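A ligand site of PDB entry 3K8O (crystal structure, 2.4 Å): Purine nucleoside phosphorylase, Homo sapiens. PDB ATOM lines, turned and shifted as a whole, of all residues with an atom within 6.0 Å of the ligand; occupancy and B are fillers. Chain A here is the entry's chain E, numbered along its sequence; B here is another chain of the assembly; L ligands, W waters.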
ATOM      1  N   SER A  33      -4.331   3.428 -16.492  1.00  0.00           N
ATOM      2  CA  SER A  33      -2.978   3.154 -17.020  1.00  0.00           C
ATOM      3  C   SER A  33      -1.876   3.558 -16.066  1.00  0.00           C
ATOM      4  O   SER A  33      -1.845   4.693 -15.597  1.00  0.00           O
ATOM      5  CB  SER A  33      -2.768   3.872 -18.347  1.00  0.00           C
ATOM      6  OG  SER A  33      -3.775   3.520 -19.257  1.00  0.00           O
ATOM      7  N   VAL A  61      -4.023  -3.655 -22.984  1.00  0.00           N
ATOM      8  CA  VAL A  61      -3.175  -2.486 -23.080  1.00  0.00           C
ATOM      9  C   VAL A  61      -2.175  -2.430 -21.913  1.00  0.00           C
ATOM     10  O   VAL A  61      -2.534  -2.729 -20.777  1.00  0.00           O
ATOM     11  CB  VAL A  61      -4.020  -1.171 -23.284  1.00  0.00           C
ATOM     12  CG1 VAL A  61      -5.518  -1.460 -23.138  1.00  0.00           C
ATOM     13  CG2 VAL A  61      -3.584  -0.041 -22.365  1.00  0.00           C
ATOM     14  N   PRO A  62      -0.907  -2.072 -22.201  1.00  0.00           N
ATOM     15  CA  PRO A  62       0.009  -1.808 -21.085  1.00  0.00           C
ATOM     16  C   PRO A  62      -0.308  -0.446 -20.444  1.00  0.00           C
ATOM     17  O   PRO A  62      -0.845   0.430 -21.126  1.00  0.00           O
ATOM     18  CB  PRO A  62       1.381  -1.773 -21.770  1.00  0.00           C
ATOM     19  CG  PRO A  62       1.095  -1.367 -23.211  1.00  0.00           C
ATOM     20  CD  PRO A  62      -0.301  -1.824 -23.528  1.00  0.00           C
ATOM     21  N   HIS A  64      -1.914  -2.384 -17.860  1.00  0.00           N
ATOM     22  CA  HIS A  64      -3.068  -2.900 -17.166  1.00  0.00           C
ATOM     23  C   HIS A  64      -2.738  -4.384 -16.913  1.00  0.00           C
ATOM     24  O   HIS A  64      -2.547  -5.151 -17.871  1.00  0.00           O
ATOM     25  CB  HIS A  64      -4.311  -2.742 -18.038  1.00  0.00           C
ATOM     26  CG  HIS A  64      -4.693  -1.325 -18.301  1.00  0.00           C
ATOM     27  ND1 HIS A  64      -5.888  -0.781 -17.887  1.00  0.00           N
ATOM     28  CD2 HIS A  64      -4.030  -0.317 -18.939  1.00  0.00           C
ATOM     29  CE1 HIS A  64      -5.952   0.486 -18.252  1.00  0.00           C
ATOM     30  NE2 HIS A  64      -4.839   0.792 -18.893  1.00  0.00           N
ATOM     31  N   HIS A  86     -11.193  -0.970 -22.303  1.00  0.00           N
ATOM     32  CA  HIS A  86     -11.534   0.177 -23.132  1.00  0.00           C
ATOM     33  C   HIS A  86     -12.333  -0.237 -24.361  1.00  0.00           C
ATOM     34  O   HIS A  86     -12.270  -1.407 -24.807  1.00  0.00           O
ATOM     35  CB  HIS A  86     -10.260   0.912 -23.540  1.00  0.00           C
ATOM     36  CG  HIS A  86      -9.348   1.235 -22.394  1.00  0.00           C
ATOM     37  ND1 HIS A  86      -8.445   0.330 -21.876  1.00  0.00           N
ATOM     38  CD2 HIS A  86      -9.187   2.379 -21.674  1.00  0.00           C
ATOM     39  CE1 HIS A  86      -7.778   0.884 -20.882  1.00  0.00           C
ATOM     40  NE2 HIS A  86      -8.209   2.129 -20.740  1.00  0.00           N
ATOM     41  N   TYR A  88     -11.838   1.052 -27.303  1.00  0.00           N
ATOM     42  CA  TYR A  88     -10.917   0.973 -28.433  1.00  0.00           C
ATOM     43  C   TYR A  88     -10.227  -0.401 -28.641  1.00  0.00           C
ATOM     44  O   TYR A  88      -9.587  -0.653 -29.672  1.00  0.00           O
ATOM     45  CB  TYR A  88      -9.896   2.104 -28.365  1.00  0.00           C
ATOM     46  CG  TYR A  88      -8.939   2.023 -27.209  1.00  0.00           C
ATOM     47  CD1 TYR A  88      -8.894   3.049 -26.248  1.00  0.00           C
ATOM     48  CD2 TYR A  88      -8.060   0.931 -27.074  1.00  0.00           C
ATOM     49  CE1 TYR A  88      -8.013   2.996 -25.185  1.00  0.00           C
ATOM     50  CE2 TYR A  88      -7.175   0.858 -26.003  1.00  0.00           C
ATOM     51  CZ  TYR A  88      -7.153   1.896 -25.063  1.00  0.00           C
ATOM     52  OH  TYR A  88      -6.277   1.834 -24.009  1.00  0.00           O
ATOM     53  N   ALA A 116      -5.386   7.803 -16.032  1.00  0.00           N
ATOM     54  CA  ALA A 116      -4.459   8.715 -16.609  1.00  0.00           C
ATOM     55  C   ALA A 116      -5.286   9.572 -17.578  1.00  0.00           C
ATOM     56  O   ALA A 116      -6.231   9.061 -18.214  1.00  0.00           O
ATOM     57  CB  ALA A 116      -3.398   7.954 -17.334  1.00  0.00           C
ATOM     58  N   ALA A 117      -4.927  10.844 -17.687  1.00  0.00           N
ATOM     59  CA  ALA A 117      -5.658  11.790 -18.529  1.00  0.00           C
ATOM     60  C   ALA A 117      -4.737  12.879 -19.042  1.00  0.00           C
ATOM     61  O   ALA A 117      -3.849  13.317 -18.322  1.00  0.00           O
ATOM     62  CB  ALA A 117      -6.817  12.401 -17.750  1.00  0.00           C
ATOM     63  N   GLY A 118      -4.943  13.320 -20.284  1.00  0.00           N
ATOM     64  CA  GLY A 118      -4.164  14.409 -20.843  1.00  0.00           C
ATOM     65  C   GLY A 118      -4.699  15.741 -20.380  1.00  0.00           C
ATOM     66  O   GLY A 118      -5.912  15.947 -20.354  1.00  0.00           O
ATOM     67  N   GLY A 119      -3.818  16.651 -20.009  1.00  0.00           N
ATOM     68  CA  GLY A 119      -4.252  17.945 -19.492  1.00  0.00           C
ATOM     69  C   GLY A 119      -4.730  18.863 -20.596  1.00  0.00           C
ATOM     70  O   GLY A 119      -4.010  19.115 -21.561  1.00  0.00           O
ATOM     71  N   TYR A 192     -13.896  15.931 -16.830  1.00  0.00           N
ATOM     72  CA  TYR A 192     -13.238  14.925 -17.670  1.00  0.00           C
ATOM     73  C   TYR A 192     -14.047  14.736 -18.944  1.00  0.00           C
ATOM     74  O   TYR A 192     -15.272  14.539 -18.887  1.00  0.00           O
ATOM     75  CB  TYR A 192     -13.139  13.622 -16.878  1.00  0.00           C
ATOM     76  CG  TYR A 192     -12.555  12.444 -17.621  1.00  0.00           C
ATOM     77  CD1 TYR A 192     -11.186  12.221 -17.657  1.00  0.00           C
ATOM     78  CD2 TYR A 192     -13.389  11.538 -18.272  1.00  0.00           C
ATOM     79  CE1 TYR A 192     -10.658  11.122 -18.338  1.00  0.00           C
ATOM     80  CE2 TYR A 192     -12.874  10.439 -18.957  1.00  0.00           C
ATOM     81  CZ  TYR A 192     -11.508  10.236 -18.979  1.00  0.00           C
ATOM     82  OH  TYR A 192     -11.009   9.137 -19.631  1.00  0.00           O
ATOM     83  N   VAL A 195     -13.280  10.456 -24.861  1.00  0.00           N
ATOM     84  CA  VAL A 195     -13.068  10.327 -26.284  1.00  0.00           C
ATOM     85  C   VAL A 195     -12.648   8.871 -26.600  1.00  0.00           C
ATOM     86  O   VAL A 195     -11.977   8.222 -25.790  1.00  0.00           O
ATOM     87  CB  VAL A 195     -12.014  11.353 -26.682  1.00  0.00           C
ATOM     88  CG1 VAL A 195     -10.793  10.729 -27.291  1.00  0.00           C
ATOM     89  CG2 VAL A 195     -12.626  12.383 -27.540  1.00  0.00           C
ATOM     90  N   PRO A 198      -8.441   4.766 -30.525  1.00  0.00           N
ATOM     91  CA  PRO A 198      -7.211   4.724 -29.740  1.00  0.00           C
ATOM     92  C   PRO A 198      -6.153   5.777 -30.092  1.00  0.00           C
ATOM     93  O   PRO A 198      -5.211   5.950 -29.333  1.00  0.00           O
ATOM     94  CB  PRO A 198      -6.646   3.312 -30.065  1.00  0.00           C
ATOM     95  CG  PRO A 198      -7.057   3.108 -31.429  1.00  0.00           C
ATOM     96  CD  PRO A 198      -8.427   3.754 -31.587  1.00  0.00           C
ATOM     97  N   PHE A 200      -4.311   9.423 -30.487  1.00  0.00           N
ATOM     98  CA  PHE A 200      -4.318  10.664 -29.744  1.00  0.00           C
ATOM     99  C   PHE A 200      -4.893  11.792 -30.579  1.00  0.00           C
ATOM    100  O   PHE A 200      -5.185  11.622 -31.754  1.00  0.00           O
ATOM    101  CB  PHE A 200      -2.927  11.023 -29.271  1.00  0.00           C
ATOM    102  CG  PHE A 200      -2.415  10.152 -28.147  1.00  0.00           C
ATOM    103  CD1 PHE A 200      -2.911  10.292 -26.861  1.00  0.00           C
ATOM    104  CD2 PHE A 200      -1.411   9.206 -28.382  1.00  0.00           C
ATOM    105  CE1 PHE A 200      -2.419   9.498 -25.835  1.00  0.00           C
ATOM    106  CE2 PHE A 200      -0.919   8.412 -27.357  1.00  0.00           C
ATOM    107  CZ  PHE A 200      -1.425   8.563 -26.087  1.00  0.00           C
ATOM    108  N   GLU A 201      -5.054  12.946 -29.941  1.00  0.00           N
ATOM    109  CA  GLU A 201      -5.857  14.038 -30.489  1.00  0.00           C
ATOM    110  C   GLU A 201      -5.007  14.996 -31.284  1.00  0.00           C
ATOM    111  O   GLU A 201      -3.813  15.137 -31.051  1.00  0.00           O
ATOM    112  CB  GLU A 201      -6.582  14.801 -29.377  1.00  0.00           C
ATOM    113  CG  GLU A 201      -7.655  14.016 -28.614  1.00  0.00           C
ATOM    114  CD  GLU A 201      -7.078  13.056 -27.558  1.00  0.00           C
ATOM    115  OE1 GLU A 201      -7.609  11.909 -27.410  1.00  0.00           O
ATOM    116  OE2 GLU A 201      -6.088  13.421 -26.879  1.00  0.00           O
ATOM    117  N   VAL A 217      -8.685  14.936 -20.730  1.00  0.00           N
ATOM    118  CA  VAL A 217      -9.220  14.026 -21.726  1.00  0.00           C
ATOM    119  C   VAL A 217      -8.626  12.634 -21.557  1.00  0.00           C
ATOM    120  O   VAL A 217      -7.430  12.493 -21.292  1.00  0.00           O
ATOM    121  CB  VAL A 217      -9.011  14.570 -23.171  1.00  0.00           C
ATOM    122  CG1 VAL A 217      -7.531  14.800 -23.509  1.00  0.00           C
ATOM    123  CG2 VAL A 217      -9.700  13.658 -24.194  1.00  0.00           C
ATOM    124  N   GLY A 218      -9.453  11.607 -21.670  1.00  0.00           N
ATOM    125  CA  GLY A 218      -8.978  10.223 -21.710  1.00  0.00           C
ATOM    126  C   GLY A 218      -9.985   9.412 -22.486  1.00  0.00           C
ATOM    127  O   GLY A 218     -10.944   9.969 -23.012  1.00  0.00           O
ATOM    128  N   MET A 219      -9.804   8.093 -22.539  1.00  0.00           N
ATOM    129  CA  MET A 219     -10.650   7.207 -23.355  1.00  0.00           C
ATOM    130  C   MET A 219     -11.242   6.103 -22.488  1.00  0.00           C
ATOM    131  O   MET A 219     -11.225   4.941 -22.872  1.00  0.00           O
ATOM    132  CB  MET A 219      -9.816   6.549 -24.461  1.00  0.00           C
ATOM    133  CG  MET A 219      -8.707   7.402 -25.020  1.00  0.00           C
ATOM    134  SD  MET A 219      -7.577   6.444 -26.043  1.00  0.00           S
ATOM    135  CE  MET A 219      -6.534   7.736 -26.689  1.00  0.00           C
ATOM    136  N   SER A 220     -11.753   6.470 -21.313  1.00  0.00           N
ATOM    137  CA  SER A 220     -12.201   5.474 -20.357  1.00  0.00           C
ATOM    138  C   SER A 220     -13.144   6.081 -19.320  1.00  0.00           C
ATOM    139  O   SER A 220     -13.582   7.213 -19.472  1.00  0.00           O
ATOM    140  CB  SER A 220     -10.995   4.875 -19.640  1.00  0.00           C
ATOM    141  OG  SER A 220     -10.596   5.698 -18.575  1.00  0.00           O
ATOM    142  N   THR A 242      -0.975  13.050 -16.726  1.00  0.00           N
ATOM    143  CA  THR A 242       0.269  12.435 -17.174  1.00  0.00           C
ATOM    144  C   THR A 242       1.016  13.244 -18.246  1.00  0.00           C
ATOM    145  O   THR A 242       2.232  13.135 -18.393  1.00  0.00           O
ATOM    146  CB  THR A 242       0.001  11.037 -17.751  1.00  0.00           C
ATOM    147  OG1 THR A 242      -1.082  11.131 -18.684  1.00  0.00           O
ATOM    148  CG2 THR A 242      -0.406  10.070 -16.643  1.00  0.00           C
ATOM    149  N   ASN A 243       0.266  14.044 -18.998  1.00  0.00           N
ATOM    150  CA  ASN A 243       0.834  14.850 -20.061  1.00  0.00           C
ATOM    151  C   ASN A 243      -0.061  16.052 -20.350  1.00  0.00           C
ATOM    152  O   ASN A 243      -1.254  16.013 -20.079  1.00  0.00           O
ATOM    153  CB  ASN A 243       0.983  14.014 -21.334  1.00  0.00           C
ATOM    154  CG  ASN A 243      -0.353  13.576 -21.869  1.00  0.00           C
ATOM    155  OD1 ASN A 243      -1.159  12.991 -21.148  1.00  0.00           O
ATOM    156  ND2 ASN A 243      -0.623  13.901 -23.119  1.00  0.00           N
ATOM    157  N   LYS A 244       0.526  17.118 -20.883  1.00  0.00           N
ATOM    158  CA  LYS A 244      -0.226  18.274 -21.362  1.00  0.00           C
ATOM    159  C   LYS A 244      -0.408  18.168 -22.870  1.00  0.00           C
ATOM    160  O   LYS A 244       0.578  18.085 -23.623  1.00  0.00           O
ATOM    161  CB  LYS A 244       0.505  19.562 -21.000  1.00  0.00           C
ATOM    162  CG  LYS A 244       0.291  20.022 -19.571  1.00  0.00           C
ATOM    163  CD  LYS A 244       0.610  21.541 -19.393  1.00  0.00           C
ATOM    164  CE  LYS A 244       2.077  21.811 -19.006  1.00  0.00           C
ATOM    165  NZ  LYS A 244       2.231  22.930 -18.018  1.00  0.00           N
ATOM    166  N   VAL A 245      -1.653  18.142 -23.318  1.00  0.00           N
ATOM    167  CA  VAL A 245      -1.940  17.865 -24.723  1.00  0.00           C
ATOM    168  C   VAL A 245      -1.433  18.984 -25.598  1.00  0.00           C
ATOM    169  O   VAL A 245      -1.431  20.165 -25.201  1.00  0.00           O
ATOM    170  CB  VAL A 245      -3.452  17.582 -25.006  1.00  0.00           C
ATOM    171  CG1 VAL A 245      -3.993  16.520 -24.050  1.00  0.00           C
ATOM    172  CG2 VAL A 245      -4.285  18.872 -24.966  1.00  0.00           C
ATOM    173  N   ALA A 255       2.078  13.240 -28.159  1.00  0.00           N
ATOM    174  CA  ALA A 255       1.580  12.390 -27.093  1.00  0.00           C
ATOM    175  C   ALA A 255       1.950  10.901 -27.314  1.00  0.00           C
ATOM    176  O   ALA A 255       1.996  10.413 -28.454  1.00  0.00           O
ATOM    177  CB  ALA A 255       0.085  12.552 -26.933  1.00  0.00           C
ATOM    178  N   ASN A 256       2.266  10.203 -26.237  1.00  0.00           N
ATOM    179  CA  ASN A 256       2.620   8.809 -26.348  1.00  0.00           C
ATOM    180  C   ASN A 256       2.373   8.084 -25.046  1.00  0.00           C
ATOM    181  O   ASN A 256       2.543   8.645 -23.954  1.00  0.00           O
ATOM    182  CB  ASN A 256       4.075   8.647 -26.820  1.00  0.00           C
ATOM    183  CG  ASN A 256       5.070   9.309 -25.900  1.00  0.00           C
ATOM    184  OD1 ASN A 256       5.298  10.516 -25.974  1.00  0.00           O
ATOM    185  ND2 ASN A 256       5.693   8.518 -25.029  1.00  0.00           N
ATOM    186  N   HIS A 257       1.971   6.826 -25.154  1.00  0.00           N
ATOM    187  CA  HIS A 257       1.690   6.000 -23.991  1.00  0.00           C
ATOM    188  C   HIS A 257       2.864   5.820 -23.036  1.00  0.00           C
ATOM    189  O   HIS A 257       2.671   5.699 -21.817  1.00  0.00           O
ATOM    190  CB  HIS A 257       1.158   4.646 -24.425  1.00  0.00           C
ATOM    191  CG  HIS A 257       0.338   3.963 -23.382  1.00  0.00           C
ATOM    192  ND1 HIS A 257      -0.775   4.544 -22.804  1.00  0.00           N
ATOM    193  CD2 HIS A 257       0.455   2.741 -22.801  1.00  0.00           C
ATOM    194  CE1 HIS A 257      -1.306   3.717 -21.937  1.00  0.00           C
ATOM    195  NE2 HIS A 257      -0.568   2.618 -21.907  1.00  0.00           N
ATOM    196  N   VAL A 260       2.852   8.499 -20.600  1.00  0.00           N
ATOM    197  CA  VAL A 260       1.742   8.367 -19.657  1.00  0.00           C
ATOM    198  C   VAL A 260       1.925   7.266 -18.620  1.00  0.00           C
ATOM    199  O   VAL A 260       1.366   7.330 -17.523  1.00  0.00           O
ATOM    200  CB  VAL A 260       0.332   8.362 -20.333  1.00  0.00           C
ATOM    201  CG1 VAL A 260       0.401   7.960 -21.778  1.00  0.00           C
ATOM    202  CG2 VAL A 260      -0.683   7.532 -19.548  1.00  0.00           C
ATOM    203  N   PHE B 159      -1.130   3.211 -29.877  1.00  0.00           N
ATOM    204  CA  PHE B 159      -1.538   4.610 -29.619  1.00  0.00           C
ATOM    205  C   PHE B 159      -0.759   5.613 -30.439  1.00  0.00           C
ATOM    206  O   PHE B 159       0.078   6.324 -29.898  1.00  0.00           O
ATOM    207  CB  PHE B 159      -1.366   4.949 -28.155  1.00  0.00           C
ATOM    208  CG  PHE B 159      -2.141   4.079 -27.210  1.00  0.00           C
ATOM    209  CD1 PHE B 159      -3.537   4.124 -27.197  1.00  0.00           C
ATOM    210  CD2 PHE B 159      -1.479   3.245 -26.330  1.00  0.00           C
ATOM    211  CE1 PHE B 159      -4.258   3.334 -26.300  1.00  0.00           C
ATOM    212  CE2 PHE B 159      -2.191   2.456 -25.438  1.00  0.00           C
ATOM    213  CZ  PHE B 159      -3.574   2.490 -25.422  1.00  0.00           C
HETATM  214  O1  LIG L   1      -2.593   6.630 -23.059  1.00  0.00           O
HETATM  215  C1  LIG L   1      -3.428   6.251 -24.150  1.00  0.00           C
HETATM  216  C2  LIG L   1      -4.681   5.548 -23.624  1.00  0.00           C
HETATM  217  O2  LIG L   1      -4.322   4.421 -22.804  1.00  0.00           O
HETATM  218  C3  LIG L   1      -5.604   6.478 -22.825  1.00  0.00           C
HETATM  219  C4  LIG L   1      -6.764   5.640 -22.293  1.00  0.00           C
HETATM  220  O3  LIG L   1      -7.898   6.456 -21.960  1.00  0.00           O
HETATM  221  N1  LIG L   1      -4.839   7.031 -21.737  1.00  0.00           N
HETATM  222  C5  LIG L   1      -5.322   8.186 -21.019  1.00  0.00           C
HETATM  223  C6  LIG L   1      -4.590   9.385 -21.542  1.00  0.00           C
HETATM  224  C7  LIG L   1      -4.966  10.210 -22.689  1.00  0.00           C
HETATM  225  N2  LIG L   1      -6.013  10.107 -23.533  1.00  0.00           N
HETATM  226  C8  LIG L   1      -6.136  11.002 -24.518  1.00  0.00           C
HETATM  227  N3  LIG L   1      -5.245  12.013 -24.697  1.00  0.00           N
HETATM  228  C9  LIG L   1      -3.430   9.964 -21.057  1.00  0.00           C
HETATM  229  N4  LIG L   1      -3.079  11.043 -21.801  1.00  0.00           N
HETATM  230  C10 LIG L   1      -3.954  11.242 -22.797  1.00  0.00           C
HETATM  231  C11 LIG L   1      -4.167  12.199 -23.922  1.00  0.00           C
HETATM  232  O4  LIG L   1      -3.375  13.146 -24.131  1.00  0.00           O
HETATM  233  O   HOH W   1      -3.211  14.326 -26.479  1.00  0.00           O
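N of Met 219 lies within hydrogen-bond range of O3 of the ligand. The side-chain carboxylate of Glu 201 sits at hydrogen-bond distance from a nitrogen (N3) of the ligand. O1 of the ligand lies within hydrogen-bond range of ND1 of His 257 (2.8 Å). The side-chain amide oxygen (OD1) of Asn 243 is in hydrogen-bond range of a nitrogen (N4) of the ligand (2.8 Å). N of Gly 118 lies close to N4 of the ligand (3.3 Å). The side-chain hydroxyl (OH) of Tyr 88 lies within hydrogen-bond range of an oxygen (O2) of the ligand (3.5 Å).
OH of Tyr 192 lies within hydrogen-bond range of N of Met 219 (3.3 Å). OD1 of Asn 243 lies within hydrogen-bond range of OG1 of Thr 242. The backbone carbonyl oxygen (O) of Asn 243 sits at hydrogen-bond distance from the backbone NH (N) of Gly 119 (2.6 Å). The backbone NH of Val 245 is in hydrogen-bond range of the backbone carbonyl oxygen of Gly 119 (3.1 Å). The backbone carbonyl oxygen (O) of Gly 218 sits at hydrogen-bond distance from the backbone NH (N) of Val 195 (3.0 Å). The backbone NH (N) of Thr 242 sits at hydrogen-bond distance from the backbone carbonyl oxygen (O) of Ala 117 (3.3 Å). A ring nitrogen (NE2) of His 64 lies within hydrogen-bond range of the side-chain hydroxyl of Ser 33 (3.0 Å). The side-chain hydroxyl (OH) of Tyr 192 lies within hydrogen-bond range of the backbone carbonyl oxygen (O) of Ser 220.
Ser 33 touches the ligand (OG to O2, 3.7 Å). Ala 116 touches the ligand. C of Ala 117 touches N4 of the ligand (3.7 Å). Phe 200 touches the ligand (CD1 to N3, 3.6 Å). Val 217 touches the ligand. CA of Gly 218 touches N2 of the ligand, at 3.5 Å. N of Ser 220 touches O3 of the ligand, at 3.9 Å. Thr 242 touches the ligand. CG1 of Val 245 touches O4 of the ligand, at 3.4 Å. Val 260 touches the ligand. Phe 159 of chain B touches the ligand (CZ to O2, 3.3 Å). Of the 28 residues printed, 17 come within 4 Å of the ligand. Along chain A the residues within 4 Å of the ligand span positions 33 to 260. The nearest printed residue that does not touch the ligand is His 86 (4.1 Å).
Water W1 bridges O4 of the ligand (2.6 Å) and OE2 of Glu 201 (3.0 Å).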
